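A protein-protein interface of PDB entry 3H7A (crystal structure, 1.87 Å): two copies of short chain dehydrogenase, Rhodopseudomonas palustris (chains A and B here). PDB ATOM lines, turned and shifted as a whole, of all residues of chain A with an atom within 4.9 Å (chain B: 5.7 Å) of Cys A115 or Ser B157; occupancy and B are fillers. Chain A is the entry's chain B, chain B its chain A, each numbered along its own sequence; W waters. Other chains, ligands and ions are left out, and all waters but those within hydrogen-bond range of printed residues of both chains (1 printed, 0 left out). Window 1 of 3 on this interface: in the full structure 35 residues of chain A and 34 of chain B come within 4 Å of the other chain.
OG of Ser B157 is in hydrogen-bond range of O of Gly A161 (2.9 Å). The side-chain hydroxyl (OG) of Ser B157 lies within hydrogen-bond range of the side-chain sulfur (SG) of Cys A115, at 3.4 Å.
Among the printed residues, pairs that only touch across the chains: Trp A111 with Phe B107, Trp A116 with Phe B107, Phe A119 with Phe B107, Ala A164 with Ala B156, Ala A164 with Ser B157, Ala A164 with Phe B160, Val A165 with Phe B107 and Val A165 with Ser B157.
Hydrophobic or aromatic side chains of chain B within 4 Å of the printed part of chain A: Phe B107, Ala B156 and Phe B160. Hydrophobic or aromatic side chains of chain A that line the printed part of chain B: Trp A111, Trp A116, Phe A119, Ala A164 and Val A165.
O of Trp A111 lies within hydrogen-bond range of N of Trp A116 (2.8 Å). The indole nitrogen (NE1) of Trp A111 lies within hydrogen-bond range of the side-chain sulfur (SG) of Cys A115, at 3.6 Å. The side-chain sulfur of Cys A115 lies within hydrogen-bond range of the backbone NH of Leu A162 (3.7 Å).
4 positions are printed for both chains. Of the 10 pairs that touch across the chains among the printed residues, none has its exchanged pair printed and touching as well.
Water W1 bridges the side-chain hydroxyl of Ser B157 (3.0 Å) and the indole nitrogen of Trp A111 (3.1 Å).
Printed residues of chain B within 4 Å of Cys A115: Ser B157 (3.4 Å). Ser B157 touches just these residues of chain A: Cys A115, Gly A161, Ala A164 and Val A165. Of the printed residues of chain B, Val A165 touches Phe B107 (3.7 Å) and Ser B157 (3.6 Å). Printed residues of chain B within 4 Å of Gly A161: Ser B157 (2.9 Å). Printed residues of chain B within 4 Å of Trp A116: Phe B107 (3.6 Å). The nearest residue of chain B that does not touch Cys A115 is Phe B107 (4.3 Å).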
ATOM      1  N   VAL A 110      33.743 -14.093   4.438  1.00  0.00           N
ATOM      2  CA  VAL A 110      32.408 -14.542   4.856  1.00  0.00           C
ATOM      3  C   VAL A 110      31.778 -13.518   5.807  1.00  0.00           C
ATOM      4  O   VAL A 110      30.607 -13.173   5.658  1.00  0.00           O
ATOM      5  CB  VAL A 110      32.446 -15.973   5.439  1.00  0.00           C
ATOM      6  CG1 VAL A 110      31.138 -16.339   6.107  1.00  0.00           C
ATOM      7  CG2 VAL A 110      32.739 -16.941   4.314  1.00  0.00           C
ATOM      8  N   TRP A 111      32.566 -12.977   6.736  1.00  0.00           N
ATOM      9  CA  TRP A 111      32.073 -11.887   7.562  1.00  0.00           C
ATOM     10  C   TRP A 111      31.681 -10.623   6.763  1.00  0.00           C
ATOM     11  O   TRP A 111      30.617 -10.027   7.010  1.00  0.00           O
ATOM     12  CB  TRP A 111      33.097 -11.526   8.622  1.00  0.00           C
ATOM     13  CG  TRP A 111      32.682 -10.337   9.436  1.00  0.00           C
ATOM     14  CD1 TRP A 111      31.801 -10.328  10.481  1.00  0.00           C
ATOM     15  CD2 TRP A 111      33.129  -8.982   9.275  1.00  0.00           C
ATOM     16  NE1 TRP A 111      31.663  -9.050  10.975  1.00  0.00           N
ATOM     17  CE2 TRP A 111      32.472  -8.207  10.262  1.00  0.00           C
ATOM     18  CE3 TRP A 111      34.026  -8.350   8.395  1.00  0.00           C
ATOM     19  CZ2 TRP A 111      32.690  -6.833  10.407  1.00  0.00           C
ATOM     20  CZ3 TRP A 111      34.244  -6.982   8.536  1.00  0.00           C
ATOM     21  CH2 TRP A 111      33.575  -6.238   9.538  1.00  0.00           C
ATOM     22  N   GLU A 112      32.527 -10.216   5.813  1.00  0.00           N
ATOM     23  CA  GLU A 112      32.253  -9.026   4.993  1.00  0.00           C
ATOM     24  C   GLU A 112      30.947  -9.159   4.220  1.00  0.00           C
ATOM     25  O   GLU A 112      30.164  -8.217   4.154  1.00  0.00           O
ATOM     26  CB  GLU A 112      33.389  -8.736   4.009  1.00  0.00           C
ATOM     27  CG  GLU A 112      34.717  -8.335   4.656  1.00  0.00           C
ATOM     28  CD  GLU A 112      35.833  -8.096   3.634  1.00  0.00           C
ATOM     29  OE1 GLU A 112      35.706  -8.510   2.453  1.00  0.00           O
ATOM     30  OE2 GLU A 112      36.842  -7.483   4.026  1.00  0.00           O
ATOM     31  N   MET A 113      30.724 -10.351   3.678  1.00  0.00           N
ATOM     32  CA  MET A 113      29.573 -10.632   2.822  1.00  0.00           C
ATOM     33  C   MET A 113      28.285 -10.855   3.633  1.00  0.00           C
ATOM     34  O   MET A 113      27.249 -10.268   3.327  1.00  0.00           O
ATOM     35  CB  MET A 113      29.897 -11.848   1.930  1.00  0.00           C
ATOM     36  CG  MET A 113      28.915 -12.168   0.800  1.00  0.00           C
ATOM     37  SD  MET A 113      29.205 -11.421  -0.836  1.00  0.00           S
ATOM     38  CE  MET A 113      28.487  -9.805  -0.627  1.00  0.00           C
ATOM     39  N   ALA A 114      28.361 -11.698   4.665  1.00  0.00           N
ATOM     40  CA  ALA A 114      27.172 -12.170   5.395  1.00  0.00           C
ATOM     41  C   ALA A 114      26.799 -11.417   6.672  1.00  0.00           C
ATOM     42  O   ALA A 114      25.720 -11.627   7.219  1.00  0.00           O
ATOM     43  CB  ALA A 114      27.326 -13.658   5.709  1.00  0.00           C
ATOM     44  N   CYS A 115      27.699 -10.581   7.169  1.00  0.00           N
ATOM     45  CA  CYS A 115      27.475  -9.914   8.432  1.00  0.00           C
ATOM     46  C   CYS A 115      27.660  -8.391   8.346  1.00  0.00           C
ATOM     47  O   CYS A 115      26.747  -7.630   8.671  1.00  0.00           O
ATOM     48  CB  CYS A 115      28.392 -10.492   9.503  1.00  0.00           C
ATOM     49  SG  CYS A 115      28.092  -9.664  11.091  1.00  0.00           S
ATOM     50  N   TRP A 116      28.849  -7.980   7.902  1.00  0.00           N
ATOM     51  CA  TRP A 116      29.211  -6.584   7.684  1.00  0.00           C
ATOM     52  C   TRP A 116      28.240  -5.951   6.709  1.00  0.00           C
ATOM     53  O   TRP A 116      27.668  -4.909   6.983  1.00  0.00           O
ATOM     54  CB  TRP A 116      30.647  -6.505   7.146  1.00  0.00           C
ATOM     55  CG  TRP A 116      31.021  -5.191   6.492  1.00  0.00           C
ATOM     56  CD1 TRP A 116      31.211  -4.959   5.156  1.00  0.00           C
ATOM     57  CD2 TRP A 116      31.254  -3.939   7.154  1.00  0.00           C
ATOM     58  NE1 TRP A 116      31.541  -3.638   4.948  1.00  0.00           N
ATOM     59  CE2 TRP A 116      31.576  -2.993   6.156  1.00  0.00           C
ATOM     60  CE3 TRP A 116      31.221  -3.527   8.492  1.00  0.00           C
ATOM     61  CZ2 TRP A 116      31.858  -1.663   6.456  1.00  0.00           C
ATOM     62  CZ3 TRP A 116      31.508  -2.209   8.789  1.00  0.00           C
ATOM     63  CH2 TRP A 116      31.821  -1.289   7.773  1.00  0.00           C
ATOM     64  N   ALA A 117      28.002  -6.629   5.599  1.00  0.00           N
ATOM     65  CA  ALA A 117      27.089  -6.118   4.586  1.00  0.00           C
ATOM     66  C   ALA A 117      25.686  -5.916   5.136  1.00  0.00           C
ATOM     67  O   ALA A 117      24.988  -4.970   4.749  1.00  0.00           O
ATOM     68  CB  ALA A 117      27.059  -7.052   3.425  1.00  0.00           C
ATOM     69  N   GLY A 118      25.282  -6.795   6.052  1.00  0.00           N
ATOM     70  CA  GLY A 118      23.990  -6.718   6.698  1.00  0.00           C
ATOM     71  C   GLY A 118      23.898  -5.573   7.661  1.00  0.00           C
ATOM     72  O   GLY A 118      22.869  -4.917   7.738  1.00  0.00           O
ATOM     73  N   PHE A 119      24.971  -5.347   8.411  1.00  0.00           N
ATOM     74  CA  PHE A 119      25.035  -4.204   9.318  1.00  0.00           C
ATOM     75  C   PHE A 119      24.887  -2.891   8.554  1.00  0.00           C
ATOM     76  O   PHE A 119      24.151  -2.006   8.986  1.00  0.00           O
ATOM     77  CB  PHE A 119      26.341  -4.208  10.118  1.00  0.00           C
ATOM     78  CG  PHE A 119      26.670  -2.870  10.757  1.00  0.00           C
ATOM     79  CD1 PHE A 119      25.935  -2.403  11.837  1.00  0.00           C
ATOM     80  CD2 PHE A 119      27.713  -2.095  10.268  1.00  0.00           C
ATOM     81  CE1 PHE A 119      26.228  -1.178  12.425  1.00  0.00           C
ATOM     82  CE2 PHE A 119      28.014  -0.862  10.839  1.00  0.00           C
ATOM     83  CZ  PHE A 119      27.269  -0.406  11.921  1.00  0.00           C
ATOM     84  N   ALA A 158      29.621 -15.440  11.104  1.00  0.00           N
ATOM     85  CA  ALA A 158      28.972 -14.357  10.379  1.00  0.00           C
ATOM     86  C   ALA A 158      27.447 -14.393  10.520  1.00  0.00           C
ATOM     87  O   ALA A 158      26.829 -13.338  10.635  1.00  0.00           O
ATOM     88  CB  ALA A 158      29.372 -14.394   8.913  1.00  0.00           C
ATOM     89  N   GLY A 161      26.568 -13.352  13.994  1.00  0.00           N
ATOM     90  CA  GLY A 161      26.852 -11.912  13.980  1.00  0.00           C
ATOM     91  C   GLY A 161      25.708 -11.122  13.370  1.00  0.00           C
ATOM     92  O   GLY A 161      25.297 -10.099  13.919  1.00  0.00           O
ATOM     93  N   LEU A 162      25.177 -11.603  12.241  1.00  0.00           N
ATOM     94  CA  LEU A 162      24.002 -10.961  11.618  1.00  0.00           C
ATOM     95  C   LEU A 162      22.750 -10.985  12.540  1.00  0.00           C
ATOM     96  O   LEU A 162      21.989  -9.999  12.636  1.00  0.00           O
ATOM     97  CB  LEU A 162      23.680 -11.621  10.253  1.00  0.00           C
ATOM     98  CG  LEU A 162      22.586 -10.895   9.452  1.00  0.00           C
ATOM     99  CD1 LEU A 162      23.090  -9.542   9.006  1.00  0.00           C
ATOM    100  CD2 LEU A 162      22.121 -11.727   8.250  1.00  0.00           C
ATOM    101  N   ALA A 164      22.672 -11.089  15.855  1.00  0.00           N
ATOM    102  CA  ALA A 164      22.838 -10.039  16.885  1.00  0.00           C
ATOM    103  C   ALA A 164      22.527  -8.633  16.391  1.00  0.00           C
ATOM    104  O   ALA A 164      21.956  -7.816  17.140  1.00  0.00           O
ATOM    105  CB  ALA A 164      24.214 -10.062  17.411  1.00  0.00           C
ATOM    106  N   VAL A 165      22.935  -8.334  15.161  1.00  0.00           N
ATOM    107  CA  VAL A 165      22.723  -7.008  14.583  1.00  0.00           C
ATOM    108  C   VAL A 165      21.217  -6.792  14.492  1.00  0.00           C
ATOM    109  O   VAL A 165      20.706  -5.768  14.952  1.00  0.00           O
ATOM    110  CB  VAL A 165      23.447  -6.849  13.204  1.00  0.00           C
ATOM    111  CG1 VAL A 165      22.919  -5.654  12.413  1.00  0.00           C
ATOM    112  CG2 VAL A 165      24.953  -6.714  13.392  1.00  0.00           C
ATOM    113  N   PHE B 107      32.252  -0.598  14.312  1.00  0.00           N
ATOM    114  CA  PHE B 107      31.776  -1.961  14.046  1.00  0.00           C
ATOM    115  C   PHE B 107      32.901  -2.908  13.652  1.00  0.00           C
ATOM    116  O   PHE B 107      32.955  -4.034  14.129  1.00  0.00           O
ATOM    117  CB  PHE B 107      30.705  -1.971  12.955  1.00  0.00           C
ATOM    118  CG  PHE B 107      29.931  -3.280  12.854  1.00  0.00           C
ATOM    119  CD1 PHE B 107      28.841  -3.525  13.680  1.00  0.00           C
ATOM    120  CD2 PHE B 107      30.285  -4.246  11.927  1.00  0.00           C
ATOM    121  CE1 PHE B 107      28.117  -4.711  13.601  1.00  0.00           C
ATOM    122  CE2 PHE B 107      29.559  -5.443  11.830  1.00  0.00           C
ATOM    123  CZ  PHE B 107      28.473  -5.670  12.668  1.00  0.00           C
ATOM    124  N   CYS B 115      36.193 -10.868  18.024  1.00  0.00           N
ATOM    125  CA  CYS B 115      35.729 -12.037  17.272  1.00  0.00           C
ATOM    126  C   CYS B 115      36.849 -12.607  16.391  1.00  0.00           C
ATOM    127  O   CYS B 115      37.268 -13.760  16.594  1.00  0.00           O
ATOM    128  CB  CYS B 115      34.518 -11.680  16.412  1.00  0.00           C
ATOM    129  SG  CYS B 115      33.890 -13.105  15.438  1.00  0.00           S
ATOM    130  N   ALA B 144      25.865 -10.262  26.108  1.00  0.00           N
ATOM    131  CA  ALA B 144      25.829  -9.861  24.697  1.00  0.00           C
ATOM    132  C   ALA B 144      26.230 -10.960  23.693  1.00  0.00           C
ATOM    133  O   ALA B 144      26.011 -10.796  22.507  1.00  0.00           O
ATOM    134  CB  ALA B 144      26.641  -8.588  24.472  1.00  0.00           C
ATOM    135  N   PHE B 152      23.746  -2.166  21.241  1.00  0.00           N
ATOM    136  CA  PHE B 152      24.837  -3.160  21.226  1.00  0.00           C
ATOM    137  C   PHE B 152      25.061  -3.893  19.912  1.00  0.00           C
ATOM    138  O   PHE B 152      25.659  -4.985  19.917  1.00  0.00           O
ATOM    139  CB  PHE B 152      24.647  -4.202  22.338  1.00  0.00           C
ATOM    140  CG  PHE B 152      24.852  -3.663  23.714  1.00  0.00           C
ATOM    141  CD1 PHE B 152      26.113  -3.287  24.142  1.00  0.00           C
ATOM    142  CD2 PHE B 152      23.782  -3.548  24.589  1.00  0.00           C
ATOM    143  CE1 PHE B 152      26.303  -2.796  25.417  1.00  0.00           C
ATOM    144  CE2 PHE B 152      23.962  -3.063  25.868  1.00  0.00           C
ATOM    145  CZ  PHE B 152      25.229  -2.684  26.284  1.00  0.00           C
ATOM    146  N   ALA B 153      24.616  -3.326  18.789  1.00  0.00           N
ATOM    147  CA  ALA B 153      24.860  -3.982  17.493  1.00  0.00           C
ATOM    148  C   ALA B 153      26.321  -4.390  17.257  1.00  0.00           C
ATOM    149  O   ALA B 153      26.578  -5.527  16.875  1.00  0.00           O
ATOM    150  CB  ALA B 153      24.333  -3.155  16.335  1.00  0.00           C
ATOM    151  N   ALA B 154      27.266  -3.489  17.518  1.00  0.00           N
ATOM    152  CA  ALA B 154      28.669  -3.782  17.288  1.00  0.00           C
ATOM    153  C   ALA B 154      29.196  -4.836  18.257  1.00  0.00           C
ATOM    154  O   ALA B 154      29.766  -5.815  17.806  1.00  0.00           O
ATOM    155  CB  ALA B 154      29.524  -2.529  17.356  1.00  0.00           C
ATOM    156  N   PHE B 155      29.005  -4.619  19.565  1.00  0.00           N
ATOM    157  CA  PHE B 155      29.479  -5.543  20.602  1.00  0.00           C
ATOM    158  C   PHE B 155      28.823  -6.925  20.526  1.00  0.00           C
ATOM    159  O   PHE B 155      29.524  -7.946  20.572  1.00  0.00           O
ATOM    160  CB  PHE B 155      29.318  -4.938  22.002  1.00  0.00           C
ATOM    161  CG  PHE B 155      29.964  -5.746  23.099  1.00  0.00           C
ATOM    162  CD1 PHE B 155      31.312  -6.082  23.037  1.00  0.00           C
ATOM    163  CD2 PHE B 155      29.222  -6.157  24.214  1.00  0.00           C
ATOM    164  CE1 PHE B 155      31.915  -6.828  24.064  1.00  0.00           C
ATOM    165  CE2 PHE B 155      29.810  -6.897  25.244  1.00  0.00           C
ATOM    166  CZ  PHE B 155      31.156  -7.233  25.166  1.00  0.00           C
ATOM    167  N   ALA B 156      27.494  -6.961  20.385  1.00  0.00           N
ATOM    168  CA  ALA B 156      26.764  -8.245  20.335  1.00  0.00           C
ATOM    169  C   ALA B 156      27.063  -9.036  19.057  1.00  0.00           C
ATOM    170  O   ALA B 156      27.138 -10.269  19.094  1.00  0.00           O
ATOM    171  CB  ALA B 156      25.255  -8.037  20.490  1.00  0.00           C
ATOM    172  N   SER B 157      27.236  -8.339  17.932  1.00  0.00           N
ATOM    173  CA  SER B 157      27.661  -8.995  16.681  1.00  0.00           C
ATOM    174  C   SER B 157      28.968  -9.762  16.852  1.00  0.00           C
ATOM    175  O   SER B 157      29.045 -10.944  16.523  1.00  0.00           O
ATOM    176  CB  SER B 157      27.796  -7.990  15.531  1.00  0.00           C
ATOM    177  OG  SER B 157      27.831  -8.675  14.286  1.00  0.00           O
ATOM    178  N   ALA B 158      29.977  -9.083  17.400  1.00  0.00           N
ATOM    179  CA  ALA B 158      31.276  -9.692  17.655  1.00  0.00           C
ATOM    180  C   ALA B 158      31.204 -10.838  18.673  1.00  0.00           C
ATOM    181  O   ALA B 158      31.868 -11.874  18.486  1.00  0.00           O
ATOM    182  CB  ALA B 158      32.279  -8.620  18.130  1.00  0.00           C
ATOM    183  N   LYS B 159      30.433 -10.650  19.758  1.00  0.00           N
ATOM    184  CA  LYS B 159      30.260 -11.670  20.812  1.00  0.00           C
ATOM    185  C   LYS B 159      29.475 -12.903  20.352  1.00  0.00           C
ATOM    186  O   LYS B 159      29.847 -14.039  20.678  1.00  0.00           O
ATOM    187  CB  LYS B 159      29.642 -11.071  22.093  1.00  0.00           C
ATOM    188  CG  LYS B 159      30.479  -9.990  22.790  1.00  0.00           C
ATOM    189  CD  LYS B 159      31.934 -10.384  23.040  1.00  0.00           C
ATOM    190  CE  LYS B 159      32.094 -11.362  24.184  1.00  0.00           C
ATOM    191  NZ  LYS B 159      33.502 -11.389  24.676  1.00  0.00           N
ATOM    192  N   PHE B 160      28.401 -12.684  19.593  1.00  0.00           N
ATOM    193  CA  PHE B 160      27.674 -13.783  18.932  1.00  0.00           C
ATOM    194  C   PHE B 160      28.628 -14.543  18.007  1.00  0.00           C
ATOM    195  O   PHE B 160      28.713 -15.777  18.054  1.00  0.00           O
ATOM    196  CB  PHE B 160      26.518 -13.244  18.085  1.00  0.00           C
ATOM    197  CG  PHE B 160      25.215 -13.112  18.820  1.00  0.00           C
ATOM    198  CD1 PHE B 160      25.090 -12.323  19.964  1.00  0.00           C
ATOM    199  CD2 PHE B 160      24.090 -13.726  18.335  1.00  0.00           C
ATOM    200  CE1 PHE B 160      23.837 -12.168  20.612  1.00  0.00           C
ATOM    201  CE2 PHE B 160      22.840 -13.588  18.970  1.00  0.00           C
ATOM    202  CZ  PHE B 160      22.726 -12.801  20.121  1.00  0.00           C
ATOM    203  N   GLY B 161      29.340 -13.779  17.178  1.00  0.00           N
ATOM    204  CA  GLY B 161      30.350 -14.300  16.278  1.00  0.00           C
ATOM    205  C   GLY B 161      31.337 -15.206  16.983  1.00  0.00           C
ATOM    206  O   GLY B 161      31.600 -16.310  16.519  1.00  0.00           O
ATOM    207  N   LEU B 162      31.856 -14.757  18.118  1.00  0.00           N
ATOM    208  CA  LEU B 162      32.808 -15.557  18.875  1.00  0.00           C
ATOM    209  C   LEU B 162      32.188 -16.830  19.464  1.00  0.00           C
ATOM    210  O   LEU B 162      32.841 -17.898  19.515  1.00  0.00           O
ATOM    211  CB  LEU B 162      33.417 -14.698  19.988  1.00  0.00           C
ATOM    212  CG  LEU B 162      34.492 -15.391  20.817  1.00  0.00           C
ATOM    213  CD1 LEU B 162      35.745 -15.546  20.029  1.00  0.00           C
ATOM    214  CD2 LEU B 162      34.728 -14.554  22.062  1.00  0.00           C
HETATM  215  O   HOH W   1      30.774  -8.363  13.832  1.00  0.00           O
